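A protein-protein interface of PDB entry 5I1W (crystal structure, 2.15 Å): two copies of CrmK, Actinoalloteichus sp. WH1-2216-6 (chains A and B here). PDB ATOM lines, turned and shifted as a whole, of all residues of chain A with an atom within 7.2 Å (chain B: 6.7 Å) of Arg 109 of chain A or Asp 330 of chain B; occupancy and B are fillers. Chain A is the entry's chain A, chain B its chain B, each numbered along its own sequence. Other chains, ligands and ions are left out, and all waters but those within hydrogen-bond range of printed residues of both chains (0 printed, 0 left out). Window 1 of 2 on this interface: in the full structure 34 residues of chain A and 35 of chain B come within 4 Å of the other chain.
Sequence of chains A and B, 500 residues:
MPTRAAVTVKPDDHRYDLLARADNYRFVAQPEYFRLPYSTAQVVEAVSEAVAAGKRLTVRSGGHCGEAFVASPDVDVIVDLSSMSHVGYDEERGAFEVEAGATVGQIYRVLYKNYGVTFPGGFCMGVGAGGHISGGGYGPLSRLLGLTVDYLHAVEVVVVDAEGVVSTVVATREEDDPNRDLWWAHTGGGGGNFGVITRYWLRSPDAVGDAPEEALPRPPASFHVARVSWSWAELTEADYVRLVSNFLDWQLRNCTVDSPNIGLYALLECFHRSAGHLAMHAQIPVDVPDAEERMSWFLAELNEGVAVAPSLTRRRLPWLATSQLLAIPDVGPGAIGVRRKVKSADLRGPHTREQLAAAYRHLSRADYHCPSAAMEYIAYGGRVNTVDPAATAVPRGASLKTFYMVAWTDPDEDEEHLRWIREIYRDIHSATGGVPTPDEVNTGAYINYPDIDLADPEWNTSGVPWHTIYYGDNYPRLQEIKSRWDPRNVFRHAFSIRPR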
ATOM      1  N   THR A 103       1.050   6.487 -26.881  1.00  0.00           N
ATOM      2  CA  THR A 103       0.516   7.204 -25.731  1.00  0.00           C
ATOM      3  C   THR A 103       0.117   8.626 -26.164  1.00  0.00           C
ATOM      4  O   THR A 103       0.716   9.198 -27.088  1.00  0.00           O
ATOM      5  CB  THR A 103       1.539   7.249 -24.590  1.00  0.00           C
ATOM      6  OG1 THR A 103       2.725   7.899 -25.052  1.00  0.00           O
ATOM      7  CG2 THR A 103       1.894   5.836 -24.125  1.00  0.00           C
ATOM      8  N   VAL A 104      -0.909   9.172 -25.519  1.00  0.00           N
ATOM      9  CA  VAL A 104      -1.435  10.504 -25.886  1.00  0.00           C
ATOM     10  C   VAL A 104      -0.369  11.599 -25.981  1.00  0.00           C
ATOM     11  O   VAL A 104      -0.424  12.409 -26.878  1.00  0.00           O
ATOM     12  CB  VAL A 104      -2.509  11.024 -24.915  1.00  0.00           C
ATOM     13  CG1 VAL A 104      -3.737  10.154 -24.970  1.00  0.00           C
ATOM     14  CG2 VAL A 104      -1.967  11.078 -23.506  1.00  0.00           C
ATOM     15  N   GLY A 105       0.589  11.594 -25.070  1.00  0.00           N
ATOM     16  CA  GLY A 105       1.576  12.652 -24.995  1.00  0.00           C
ATOM     17  C   GLY A 105       2.460  12.624 -26.215  1.00  0.00           C
ATOM     18  O   GLY A 105       2.847  13.658 -26.743  1.00  0.00           O
ATOM     19  N   GLN A 106       2.788  11.437 -26.667  1.00  0.00           N
ATOM     20  CA  GLN A 106       3.633  11.301 -27.826  1.00  0.00           C
ATOM     21  C   GLN A 106       2.826  11.700 -29.046  1.00  0.00           C
ATOM     22  O   GLN A 106       3.301  12.414 -29.912  1.00  0.00           O
ATOM     23  CB  GLN A 106       4.164   9.873 -27.947  1.00  0.00           C
ATOM     24  CG  GLN A 106       4.371   9.390 -29.374  1.00  0.00           C
ATOM     25  CD  GLN A 106       4.364   7.854 -29.504  1.00  0.00           C
ATOM     26  OE1 GLN A 106       4.032   7.115 -28.546  1.00  0.00           O
ATOM     27  NE2 GLN A 106       4.729   7.367 -30.708  1.00  0.00           N
ATOM     28  N   ILE A 107       1.581  11.285 -29.084  1.00  0.00           N
ATOM     29  CA  ILE A 107       0.713  11.613 -30.214  1.00  0.00           C
ATOM     30  C   ILE A 107       0.603  13.133 -30.421  1.00  0.00           C
ATOM     31  O   ILE A 107       0.733  13.598 -31.552  1.00  0.00           O
ATOM     32  CB  ILE A 107      -0.699  11.038 -29.988  1.00  0.00           C
ATOM     33  CG1 ILE A 107      -0.636   9.498 -30.014  1.00  0.00           C
ATOM     34  CG2 ILE A 107      -1.671  11.535 -31.035  1.00  0.00           C
ATOM     35  CD1 ILE A 107      -1.937   8.848 -29.581  1.00  0.00           C
ATOM     36  N   TYR A 108       0.347  13.880 -29.333  1.00  0.00           N
ATOM     37  CA  TYR A 108       0.186  15.282 -29.422  1.00  0.00           C
ATOM     38  C   TYR A 108       1.433  15.891 -29.997  1.00  0.00           C
ATOM     39  O   TYR A 108       1.313  16.806 -30.777  1.00  0.00           O
ATOM     40  CB  TYR A 108      -0.093  15.946 -28.054  1.00  0.00           C
ATOM     41  CG  TYR A 108      -1.445  15.674 -27.476  1.00  0.00           C
ATOM     42  CD1 TYR A 108      -2.551  15.480 -28.291  1.00  0.00           C
ATOM     43  CD2 TYR A 108      -1.625  15.606 -26.100  1.00  0.00           C
ATOM     44  CE1 TYR A 108      -3.794  15.196 -27.756  1.00  0.00           C
ATOM     45  CE2 TYR A 108      -2.868  15.333 -25.548  1.00  0.00           C
ATOM     46  CZ  TYR A 108      -3.966  15.131 -26.377  1.00  0.00           C
ATOM     47  OH  TYR A 108      -5.237  14.844 -25.848  1.00  0.00           O
ATOM     48  N   ARG A 109       2.618  15.413 -29.586  1.00  0.00           N
ATOM     49  CA  ARG A 109       3.874  16.038 -29.986  1.00  0.00           C
ATOM     50  C   ARG A 109       4.102  15.822 -31.447  1.00  0.00           C
ATOM     51  O   ARG A 109       4.493  16.735 -32.143  1.00  0.00           O
ATOM     52  CB  ARG A 109       5.091  15.472 -29.247  1.00  0.00           C
ATOM     53  CG  ARG A 109       5.185  15.820 -27.771  1.00  0.00           C
ATOM     54  CD  ARG A 109       6.404  15.147 -27.126  1.00  0.00           C
ATOM     55  NE  ARG A 109       6.637  15.663 -25.770  1.00  0.00           N
ATOM     56  CZ  ARG A 109       6.360  15.021 -24.628  1.00  0.00           C
ATOM     57  NH1 ARG A 109       5.828  13.797 -24.632  1.00  0.00           N
ATOM     58  NH2 ARG A 109       6.618  15.610 -23.459  1.00  0.00           N
ATOM     59  N   VAL A 110       3.900  14.601 -31.905  1.00  0.00           N
ATOM     60  CA  VAL A 110       4.176  14.264 -33.284  1.00  0.00           C
ATOM     61  C   VAL A 110       3.209  14.998 -34.203  1.00  0.00           C
ATOM     62  O   VAL A 110       3.629  15.593 -35.176  1.00  0.00           O
ATOM     63  CB  VAL A 110       4.049  12.750 -33.531  1.00  0.00           C
ATOM     64  CG1 VAL A 110       4.234  12.440 -35.002  1.00  0.00           C
ATOM     65  CG2 VAL A 110       5.086  11.983 -32.715  1.00  0.00           C
ATOM     66  N   LEU A 111       1.906  14.952 -33.907  1.00  0.00           N
ATOM     67  CA  LEU A 111       0.924  15.607 -34.767  1.00  0.00           C
ATOM     68  C   LEU A 111       1.154  17.095 -34.864  1.00  0.00           C
ATOM     69  O   LEU A 111       1.045  17.672 -35.947  1.00  0.00           O
ATOM     70  CB  LEU A 111      -0.491  15.384 -34.265  1.00  0.00           C
ATOM     71  CG  LEU A 111      -1.038  13.966 -34.345  1.00  0.00           C
ATOM     72  CD1 LEU A 111      -2.481  13.989 -33.856  1.00  0.00           C
ATOM     73  CD2 LEU A 111      -0.927  13.406 -35.745  1.00  0.00           C
ATOM     74  N   TYR A 112       1.479  17.710 -33.724  1.00  0.00           N
ATOM     75  CA  TYR A 112       1.582  19.121 -33.664  1.00  0.00           C
ATOM     76  C   TYR A 112       2.863  19.662 -34.283  1.00  0.00           C
ATOM     77  O   TYR A 112       2.812  20.532 -35.154  1.00  0.00           O
ATOM     78  CB  TYR A 112       1.453  19.651 -32.211  1.00  0.00           C
ATOM     79  CG  TYR A 112       1.365  21.146 -32.260  1.00  0.00           C
ATOM     80  CD1 TYR A 112       0.253  21.746 -32.785  1.00  0.00           C
ATOM     81  CD2 TYR A 112       2.417  21.952 -31.880  1.00  0.00           C
ATOM     82  CE1 TYR A 112       0.136  23.125 -32.846  1.00  0.00           C
ATOM     83  CE2 TYR A 112       2.329  23.352 -31.983  1.00  0.00           C
ATOM     84  CZ  TYR A 112       1.178  23.924 -32.459  1.00  0.00           C
ATOM     85  OH  TYR A 112       1.037  25.289 -32.590  1.00  0.00           O
ATOM     86  N   LYS A 113       4.013  19.186 -33.829  1.00  0.00           N
ATOM     87  CA  LYS A 113       5.283  19.642 -34.401  1.00  0.00           C
ATOM     88  C   LYS A 113       5.387  19.345 -35.896  1.00  0.00           C
ATOM     89  O   LYS A 113       5.874  20.166 -36.644  1.00  0.00           O
ATOM     90  CB  LYS A 113       6.497  19.053 -33.670  1.00  0.00           C
ATOM     91  CG  LYS A 113       6.612  19.509 -32.223  1.00  0.00           C
ATOM     92  CD  LYS A 113       7.861  18.919 -31.531  1.00  0.00           C
ATOM     93  CE  LYS A 113       7.951  19.398 -30.097  1.00  0.00           C
ATOM     94  NZ  LYS A 113       9.029  18.738 -29.292  1.00  0.00           N
ATOM     95  N   ASN A 114       4.944  18.190 -36.331  1.00  0.00           N
ATOM     96  CA  ASN A 114       5.177  17.819 -37.727  1.00  0.00           C
ATOM     97  C   ASN A 114       4.138  18.384 -38.679  1.00  0.00           C
ATOM     98  O   ASN A 114       4.412  18.617 -39.827  1.00  0.00           O
ATOM     99  CB  ASN A 114       5.186  16.327 -37.882  1.00  0.00           C
ATOM    100  CG  ASN A 114       6.390  15.715 -37.250  1.00  0.00           C
ATOM    101  OD1 ASN A 114       7.470  15.962 -37.669  1.00  0.00           O
ATOM    102  ND2 ASN A 114       6.194  14.912 -36.247  1.00  0.00           N
ATOM    103  N   TYR A 115       2.939  18.593 -38.195  1.00  0.00           N
ATOM    104  CA  TYR A 115       1.843  18.977 -39.061  1.00  0.00           C
ATOM    105  C   TYR A 115       1.077  20.167 -38.583  1.00  0.00           C
ATOM    106  O   TYR A 115       0.293  20.673 -39.323  1.00  0.00           O
ATOM    107  CB  TYR A 115       0.883  17.806 -39.136  1.00  0.00           C
ATOM    108  CG  TYR A 115       1.524  16.528 -39.592  1.00  0.00           C
ATOM    109  CD1 TYR A 115       1.756  16.272 -40.955  1.00  0.00           C
ATOM    110  CD2 TYR A 115       1.820  15.563 -38.699  1.00  0.00           C
ATOM    111  CE1 TYR A 115       2.316  15.065 -41.379  1.00  0.00           C
ATOM    112  CE2 TYR A 115       2.376  14.350 -39.095  1.00  0.00           C
ATOM    113  CZ  TYR A 115       2.636  14.117 -40.426  1.00  0.00           C
ATOM    114  OH  TYR A 115       3.141  12.883 -40.733  1.00  0.00           O
ATOM    115  N   VAL A 117      -1.318  20.154 -36.210  1.00  0.00           N
ATOM    116  CA  VAL A 117      -2.679  19.802 -35.862  1.00  0.00           C
ATOM    117  C   VAL A 117      -2.757  19.122 -34.512  1.00  0.00           C
ATOM    118  O   VAL A 117      -1.751  18.757 -33.913  1.00  0.00           O
ATOM    119  CB  VAL A 117      -3.310  18.874 -36.894  1.00  0.00           C
ATOM    120  CG1 VAL A 117      -3.349  19.564 -38.224  1.00  0.00           C
ATOM    121  CG2 VAL A 117      -2.552  17.578 -37.020  1.00  0.00           C
ATOM    122  N   THR A 118      -3.977  18.920 -34.064  1.00  0.00           N
ATOM    123  CA  THR A 118      -4.202  18.136 -32.922  1.00  0.00           C
ATOM    124  C   THR A 118      -5.593  17.474 -32.930  1.00  0.00           C
ATOM    125  O   THR A 118      -6.406  17.716 -33.820  1.00  0.00           O
ATOM    126  CB  THR A 118      -4.034  19.024 -31.663  1.00  0.00           C
ATOM    127  OG1 THR A 118      -3.851  18.184 -30.497  1.00  0.00           O
ATOM    128  CG2 THR A 118      -5.215  19.940 -31.495  1.00  0.00           C
ATOM    129  N   MET A 125      -0.332  11.732 -19.695  1.00  0.00           N
ATOM    130  CA  MET A 125       0.722  11.512 -20.724  1.00  0.00           C
ATOM    131  C   MET A 125       0.989  10.096 -21.207  1.00  0.00           C
ATOM    132  O   MET A 125       1.333   9.884 -22.398  1.00  0.00           O
ATOM    133  CB  MET A 125       2.065  12.038 -20.183  1.00  0.00           C
ATOM    134  CG  MET A 125       2.118  13.549 -20.165  1.00  0.00           C
ATOM    135  SD  MET A 125       1.865  14.237 -21.828  1.00  0.00           S
ATOM    136  CE  MET A 125       3.504  13.882 -22.489  1.00  0.00           C
ATOM    137  N   TRP A 319      -0.104  26.623 -27.160  1.00  0.00           N
ATOM    138  CA  TRP A 319      -1.013  25.536 -26.839  1.00  0.00           C
ATOM    139  C   TRP A 319      -0.319  24.295 -26.286  1.00  0.00           C
ATOM    140  O   TRP A 319      -0.701  23.784 -25.238  1.00  0.00           O
ATOM    141  CB  TRP A 319      -1.903  25.169 -28.027  1.00  0.00           C
ATOM    142  CG  TRP A 319      -2.554  23.925 -27.712  1.00  0.00           C
ATOM    143  CD1 TRP A 319      -3.548  23.719 -26.790  1.00  0.00           C
ATOM    144  CD2 TRP A 319      -2.178  22.642 -28.219  1.00  0.00           C
ATOM    145  NE1 TRP A 319      -3.829  22.361 -26.723  1.00  0.00           N
ATOM    146  CE2 TRP A 319      -3.001  21.690 -27.595  1.00  0.00           C
ATOM    147  CE3 TRP A 319      -1.224  22.216 -29.150  1.00  0.00           C
ATOM    148  CZ2 TRP A 319      -2.901  20.335 -27.875  1.00  0.00           C
ATOM    149  CZ3 TRP A 319      -1.135  20.880 -29.453  1.00  0.00           C
ATOM    150  CH2 TRP A 319      -1.963  19.950 -28.811  1.00  0.00           C
ATOM    151  N   LEU A 320       0.706  23.815 -26.981  1.00  0.00           N
ATOM    152  CA  LEU A 320       1.281  22.530 -26.631  1.00  0.00           C
ATOM    153  C   LEU A 320       1.884  22.639 -25.244  1.00  0.00           C
ATOM    154  O   LEU A 320       1.794  21.727 -24.479  1.00  0.00           O
ATOM    155  CB  LEU A 320       2.298  22.057 -27.640  1.00  0.00           C
ATOM    156  CG  LEU A 320       2.940  20.700 -27.275  1.00  0.00           C
ATOM    157  CD1 LEU A 320       1.917  19.575 -27.306  1.00  0.00           C
ATOM    158  CD2 LEU A 320       4.114  20.342 -28.192  1.00  0.00           C
ATOM    159  N   GLN A 324       1.036  20.644 -21.840  1.00  0.00           N
ATOM    160  CA  GLN A 324       1.984  19.900 -21.025  1.00  0.00           C
ATOM    161  C   GLN A 324       2.025  20.412 -19.560  1.00  0.00           C
ATOM    162  O   GLN A 324       2.344  19.661 -18.636  1.00  0.00           O
ATOM    163  CB  GLN A 324       3.359  19.878 -21.678  1.00  0.00           C
ATOM    164  CG  GLN A 324       3.351  19.090 -23.000  1.00  0.00           C
ATOM    165  CD  GLN A 324       4.613  19.238 -23.831  1.00  0.00           C
ATOM    166  OE1 GLN A 324       5.321  20.239 -23.768  1.00  0.00           O
ATOM    167  NE2 GLN A 324       4.879  18.240 -24.647  1.00  0.00           N
ATOM    168  N   LEU A 325       1.644  21.657 -19.357  1.00  0.00           N
ATOM    169  CA  LEU A 325       1.642  22.244 -18.002  1.00  0.00           C
ATOM    170  C   LEU A 325       0.633  21.524 -17.123  1.00  0.00           C
ATOM    171  O   LEU A 325       0.948  21.031 -16.043  1.00  0.00           O
ATOM    172  CB  LEU A 325       1.345  23.753 -18.062  1.00  0.00           C
ATOM    173  CG  LEU A 325       1.196  24.502 -16.720  1.00  0.00           C
ATOM    174  CD1 LEU A 325       2.545  24.611 -16.026  1.00  0.00           C
ATOM    175  CD2 LEU A 325       0.617  25.883 -16.948  1.00  0.00           C
ATOM    176  N   PRO A 329       2.165  13.779 -15.119  1.00  0.00           N
ATOM    177  CA  PRO A 329       3.383  13.064 -15.470  1.00  0.00           C
ATOM    178  C   PRO A 329       3.201  11.570 -15.447  1.00  0.00           C
ATOM    179  O   PRO A 329       2.532  11.044 -14.567  1.00  0.00           O
ATOM    180  CB  PRO A 329       4.377  13.439 -14.357  1.00  0.00           C
ATOM    181  CG  PRO A 329       3.646  14.277 -13.375  1.00  0.00           C
ATOM    182  CD  PRO A 329       2.325  14.646 -13.936  1.00  0.00           C
ATOM    183  N   ASP A 330       3.863  10.927 -16.394  1.00  0.00           N
ATOM    184  CA  ASP A 330       4.013   9.482 -16.476  1.00  0.00           C
ATOM    185  C   ASP A 330       5.170   8.894 -15.581  1.00  0.00           C
ATOM    186  O   ASP A 330       5.189   7.684 -15.383  1.00  0.00           O
ATOM    187  CB  ASP A 330       4.290   9.131 -17.959  1.00  0.00           C
ATOM    188  CG  ASP A 330       5.420  10.032 -18.577  1.00  0.00           C
ATOM    189  OD1 ASP A 330       5.240  11.292 -18.655  1.00  0.00           O
ATOM    190  OD2 ASP A 330       6.499   9.482 -18.934  1.00  0.00           O
ATOM    191  N   VAL A 331       6.132   9.720 -15.114  1.00  0.00           N
ATOM    192  CA  VAL A 331       7.214   9.264 -14.184  1.00  0.00           C
ATOM    193  C   VAL A 331       7.215  10.052 -12.884  1.00  0.00           C
ATOM    194  O   VAL A 331       6.426  10.967 -12.733  1.00  0.00           O
ATOM    195  CB  VAL A 331       8.607   9.372 -14.816  1.00  0.00           C
ATOM    196  CG1 VAL A 331       8.701   8.468 -16.046  1.00  0.00           C
ATOM    197  CG2 VAL A 331       8.915  10.823 -15.166  1.00  0.00           C
ATOM    198  N   HIS B  64      17.378  20.467 -23.584  1.00  0.00           N
ATOM    199  CA  HIS B  64      17.750  20.449 -22.180  1.00  0.00           C
ATOM    200  C   HIS B  64      18.948  21.262 -21.786  1.00  0.00           C
ATOM    201  O   HIS B  64      19.280  21.346 -20.586  1.00  0.00           O
ATOM    202  CB  HIS B  64      17.862  19.023 -21.671  1.00  0.00           C
ATOM    203  CG  HIS B  64      16.574  18.582 -21.096  1.00  0.00           C
ATOM    204  ND1 HIS B  64      16.219  18.897 -19.805  1.00  0.00           N
ATOM    205  CD2 HIS B  64      15.464  18.077 -21.681  1.00  0.00           C
ATOM    206  CE1 HIS B  64      14.978  18.500 -19.581  1.00  0.00           C
ATOM    207  NE2 HIS B  64      14.505  17.989 -20.704  1.00  0.00           N
ATOM    208  N   THR B 103      14.596  10.483 -26.837  1.00  0.00           N
ATOM    209  CA  THR B 103      14.783  10.952 -25.468  1.00  0.00           C
ATOM    210  C   THR B 103      15.137   9.780 -24.578  1.00  0.00           C
ATOM    211  O   THR B 103      14.664   8.671 -24.816  1.00  0.00           O
ATOM    212  CB  THR B 103      13.515  11.628 -24.914  1.00  0.00           C
ATOM    213  OG1 THR B 103      12.435  10.692 -24.922  1.00  0.00           O
ATOM    214  CG2 THR B 103      13.115  12.851 -25.734  1.00  0.00           C
ATOM    215  N   ARG B 109      12.728   2.521 -22.205  1.00  0.00           N
ATOM    216  CA  ARG B 109      11.537   1.717 -22.364  1.00  0.00           C
ATOM    217  C   ARG B 109      11.676   0.772 -23.519  1.00  0.00           C
ATOM    218  O   ARG B 109      11.386  -0.419 -23.357  1.00  0.00           O
ATOM    219  CB  ARG B 109      10.296   2.571 -22.573  1.00  0.00           C
ATOM    220  CG  ARG B 109       9.787   3.252 -21.319  1.00  0.00           C
ATOM    221  CD  ARG B 109       8.483   3.961 -21.668  1.00  0.00           C
ATOM    222  NE  ARG B 109       8.015   4.836 -20.598  1.00  0.00           N
ATOM    223  CZ  ARG B 109       8.134   6.166 -20.591  1.00  0.00           C
ATOM    224  NH1 ARG B 109       8.723   6.807 -21.606  1.00  0.00           N
ATOM    225  NH2 ARG B 109       7.671   6.867 -19.551  1.00  0.00           N
ATOM    226  N   CYS B 124      16.593  12.068 -16.004  1.00  0.00           N
ATOM    227  CA  CYS B 124      15.559  12.949 -16.545  1.00  0.00           C
ATOM    228  C   CYS B 124      14.923  12.459 -17.877  1.00  0.00           C
ATOM    229  O   CYS B 124      15.609  12.069 -18.831  1.00  0.00           O
ATOM    230  CB  CYS B 124      16.147  14.335 -16.697  1.00  0.00           C
ATOM    231  SG  CYS B 124      16.853  15.039 -15.149  1.00  0.00           S
ATOM    232  N   MET B 125      13.602  12.481 -17.926  1.00  0.00           N
ATOM    233  CA  MET B 125      12.869  11.826 -19.010  1.00  0.00           C
ATOM    234  C   MET B 125      13.052  12.387 -20.406  1.00  0.00           C
ATOM    235  O   MET B 125      13.291  11.640 -21.329  1.00  0.00           O
ATOM    236  CB  MET B 125      11.389  11.822 -18.687  1.00  0.00           C
ATOM    237  CG  MET B 125      11.036  10.721 -17.707  1.00  0.00           C
ATOM    238  SD  MET B 125      11.354   9.046 -18.314  1.00  0.00           S
ATOM    239  CE  MET B 125      10.099   9.006 -19.608  1.00  0.00           C
ATOM    240  N   GLY B 126      12.922  13.700 -20.550  1.00  0.00           N
ATOM    241  CA  GLY B 126      12.959  14.359 -21.858  1.00  0.00           C
ATOM    242  C   GLY B 126      14.326  14.819 -22.356  1.00  0.00           C
ATOM    243  O   GLY B 126      14.397  15.533 -23.330  1.00  0.00           O
ATOM    244  N   VAL B 127      15.404  14.393 -21.713  1.00  0.00           N
ATOM    245  CA  VAL B 127      16.763  14.727 -22.132  1.00  0.00           C
ATOM    246  C   VAL B 127      16.966  13.979 -23.474  1.00  0.00           C
ATOM    247  O   VAL B 127      16.521  12.850 -23.611  1.00  0.00           O
ATOM    248  CB  VAL B 127      17.724  14.237 -21.051  1.00  0.00           C
ATOM    249  CG1 VAL B 127      19.156  14.076 -21.545  1.00  0.00           C
ATOM    250  CG2 VAL B 127      17.666  15.146 -19.846  1.00  0.00           C
ATOM    251  N   ILE B 328      12.875  12.736 -13.445  1.00  0.00           N
ATOM    252  CA  ILE B 328      12.199  14.007 -13.422  1.00  0.00           C
ATOM    253  C   ILE B 328      11.281  14.042 -14.634  1.00  0.00           C
ATOM    254  O   ILE B 328      11.719  13.706 -15.739  1.00  0.00           O
ATOM    255  CB  ILE B 328      13.217  15.169 -13.464  1.00  0.00           C
ATOM    256  CG1 ILE B 328      13.784  15.389 -12.053  1.00  0.00           C
ATOM    257  CG2 ILE B 328      12.601  16.448 -14.004  1.00  0.00           C
ATOM    258  CD1 ILE B 328      14.938  14.469 -11.767  1.00  0.00           C
ATOM    259  N   PRO B 329      10.001  14.406 -14.406  1.00  0.00           N
ATOM    260  CA  PRO B 329       8.969  14.519 -15.412  1.00  0.00           C
ATOM    261  C   PRO B 329       9.297  15.569 -16.420  1.00  0.00           C
ATOM    262  O   PRO B 329       9.862  16.603 -16.069  1.00  0.00           O
ATOM    263  CB  PRO B 329       7.757  15.037 -14.649  1.00  0.00           C
ATOM    264  CG  PRO B 329       8.117  15.127 -13.205  1.00  0.00           C
ATOM    265  CD  PRO B 329       9.488  14.594 -13.026  1.00  0.00           C
ATOM    266  N   ASP B 330       8.861  15.318 -17.647  1.00  0.00           N
ATOM    267  CA  ASP B 330       8.987  16.244 -18.780  1.00  0.00           C
ATOM    268  C   ASP B 330       7.682  17.056 -19.018  1.00  0.00           C
ATOM    269  O   ASP B 330       7.554  17.761 -20.019  1.00  0.00           O
ATOM    270  CB  ASP B 330       9.399  15.463 -20.050  1.00  0.00           C
ATOM    271  CG  ASP B 330       8.607  14.136 -20.237  1.00  0.00           C
ATOM    272  OD1 ASP B 330       8.456  13.330 -19.261  1.00  0.00           O
ATOM    273  OD2 ASP B 330       8.144  13.903 -21.372  1.00  0.00           O
ATOM    274  N   VAL B 331       6.717  16.944 -18.103  1.00  0.00           N
ATOM    275  CA  VAL B 331       5.501  17.751 -18.152  1.00  0.00           C
ATOM    276  C   VAL B 331       5.084  18.118 -16.759  1.00  0.00           C
ATOM    277  O   VAL B 331       5.580  17.569 -15.817  1.00  0.00           O
ATOM    278  CB  VAL B 331       4.355  17.006 -18.839  1.00  0.00           C
ATOM    279  CG1 VAL B 331       4.723  16.716 -20.275  1.00  0.00           C
ATOM    280  CG2 VAL B 331       4.024  15.713 -18.100  1.00  0.00           C
ATOM    281  N   GLY B 332       4.133  19.016 -16.639  1.00  0.00           N
ATOM    282  CA  GLY B 332       3.680  19.463 -15.330  1.00  0.00           C
ATOM    283  C   GLY B 332       4.398  20.738 -14.912  1.00  0.00           C
ATOM    284  O   GLY B 332       5.319  21.214 -15.621  1.00  0.00           O
ATOM    285  N   ALA B 335       8.216  21.134 -14.972  1.00  0.00           N
ATOM    286  CA  ALA B 335       8.967  21.035 -16.233  1.00  0.00           C
ATOM    287  C   ALA B 335       8.670  22.125 -17.218  1.00  0.00           C
ATOM    288  O   ALA B 335       9.509  22.412 -18.061  1.00  0.00           O
ATOM    289  CB  ALA B 335       8.730  19.685 -16.908  1.00  0.00           C
ATOM    290  N   ILE B 336       7.494  22.732 -17.148  1.00  0.00           N
ATOM    291  CA  ILE B 336       7.048  23.539 -18.271  1.00  0.00           C
ATOM    292  C   ILE B 336       6.896  25.000 -17.883  1.00  0.00           C
ATOM    293  O   ILE B 336       6.171  25.324 -16.951  1.00  0.00           O
ATOM    294  CB  ILE B 336       5.695  23.044 -18.819  1.00  0.00           C
ATOM    295  CG1 ILE B 336       5.756  21.549 -19.217  1.00  0.00           C
ATOM    296  CG2 ILE B 336       5.263  23.911 -19.994  1.00  0.00           C
ATOM    297  CD1 ILE B 336       6.725  21.188 -20.339  1.00  0.00           C
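Hydrophobic or aromatic side chains of chain A within 4 Å of the printed part of chain B: Met 125, Leu 325, Pro 329 and Val 331. Along chain A the printed residues that touch a printed residue of chain B span positions 109 to 331. Printed residues of chain B that touch a printed residue of chain A: Arg 109, Met 125, Pro 329, Asp 330, Val 331, Gly 332 and Ile 336. Among the printed residues, 16 pairs touch across the chains. Among the printed residues, Asp or Glu carboxylates within 4 Å of a Lys or Arg side-chain nitrogen of the other chain: Arg 109 of chain A with Asp 330 of chain B and Asp 330 of chain A with Arg 109 of chain B.
Arg 109 of chain A touches Val 331 of chain B, and with the chains exchanged Val 331 of chain A touches Arg 109 of chain B. Met 125 of chain A touches Val 331 of chain B, and with the chains exchanged Val 331 of chain A touches Met 125 of chain B. Asp 330 of chain A touches Met 125 of chain B, but with the chains exchanged Met 125 of chain A does not touch Asp 330 of chain B (4.8 Å). Of the 16 pairs that touch across the chains among the printed residues, 10 have their exchanged pair printed and touching as well.
Arg 109 of chain A touches just these residues of chain B: Asp 330 (3.1 Å) and Val 331 (3.9 Å). Of the printed residues of chain B, Asp 330 of chain A touches Arg 109, Met 125 and Asp 330. Asp 330 of chain B touches two residues of chain A. Printed residues of chain A within 4 Å of Ile 336 of chain B: Gln 324 (3.8 Å) and Leu 325 (3.8 Å). The nearest residue of chain B that does not touch Arg 109 of chain A is Ile 336 of chain B (6.4 Å). The nearest residue of chain A that does not touch Asp 330 of chain B is Met 125 of chain A (4.8 Å).
Arg 109 of chain A touches Val 331 of chain B. Val 331 of chain B touches Met 125 of chain A. Gln 324 of chain A touches Ile 336 of chain B. CD1 of Leu 325 of chain A touches O of Ile 336 of chain B (3.8 Å). Pro 329 of chain B touches Pro 329 of chain A. CG2 of Val 331 of chain B touches CA of Pro 329 of chain A (3.8 Å). Asp 330 of chain A touches Met 125 of chain B (OD2 to CE, 3.7 Å). Val 331 of chain A touches Met 125 of chain B (CG2 to CG, 3.3 Å). Pro 329 of chain B touches Val 331 of chain A (CA to CG2, 3.7 Å).
The side-chain carboxylate (OD2) of Asp 330 of chain A is in salt-bridge range of the guanidinium group (NH2) of Arg 109 of chain B. The backbone carbonyl oxygen (O) of Gln 324 of chain A sits at hydrogen-bond distance from the backbone NH (N) of Gly 332 of chain B. The guanidinium group (NH2) of Arg 109 of chain A lies within salt-bridge range of the side-chain carboxylate (OD2) of Asp 330 of chain B (3.1 Å).
The backbone NH (N) of Gly 105 of chain A is in hydrogen-bond range of the backbone carbonyl oxygen (O) of Met 125 of chain A, 3.3 Å away. The backbone carbonyl oxygen (O) of Ile 328 of chain B lies within hydrogen-bond range of the backbone NH (N) of Met 125 of chain B, at 3.1 Å. NE of Arg 109 of chain A lies close to NE2 of Gln 324 of chain A (3.3 Å).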
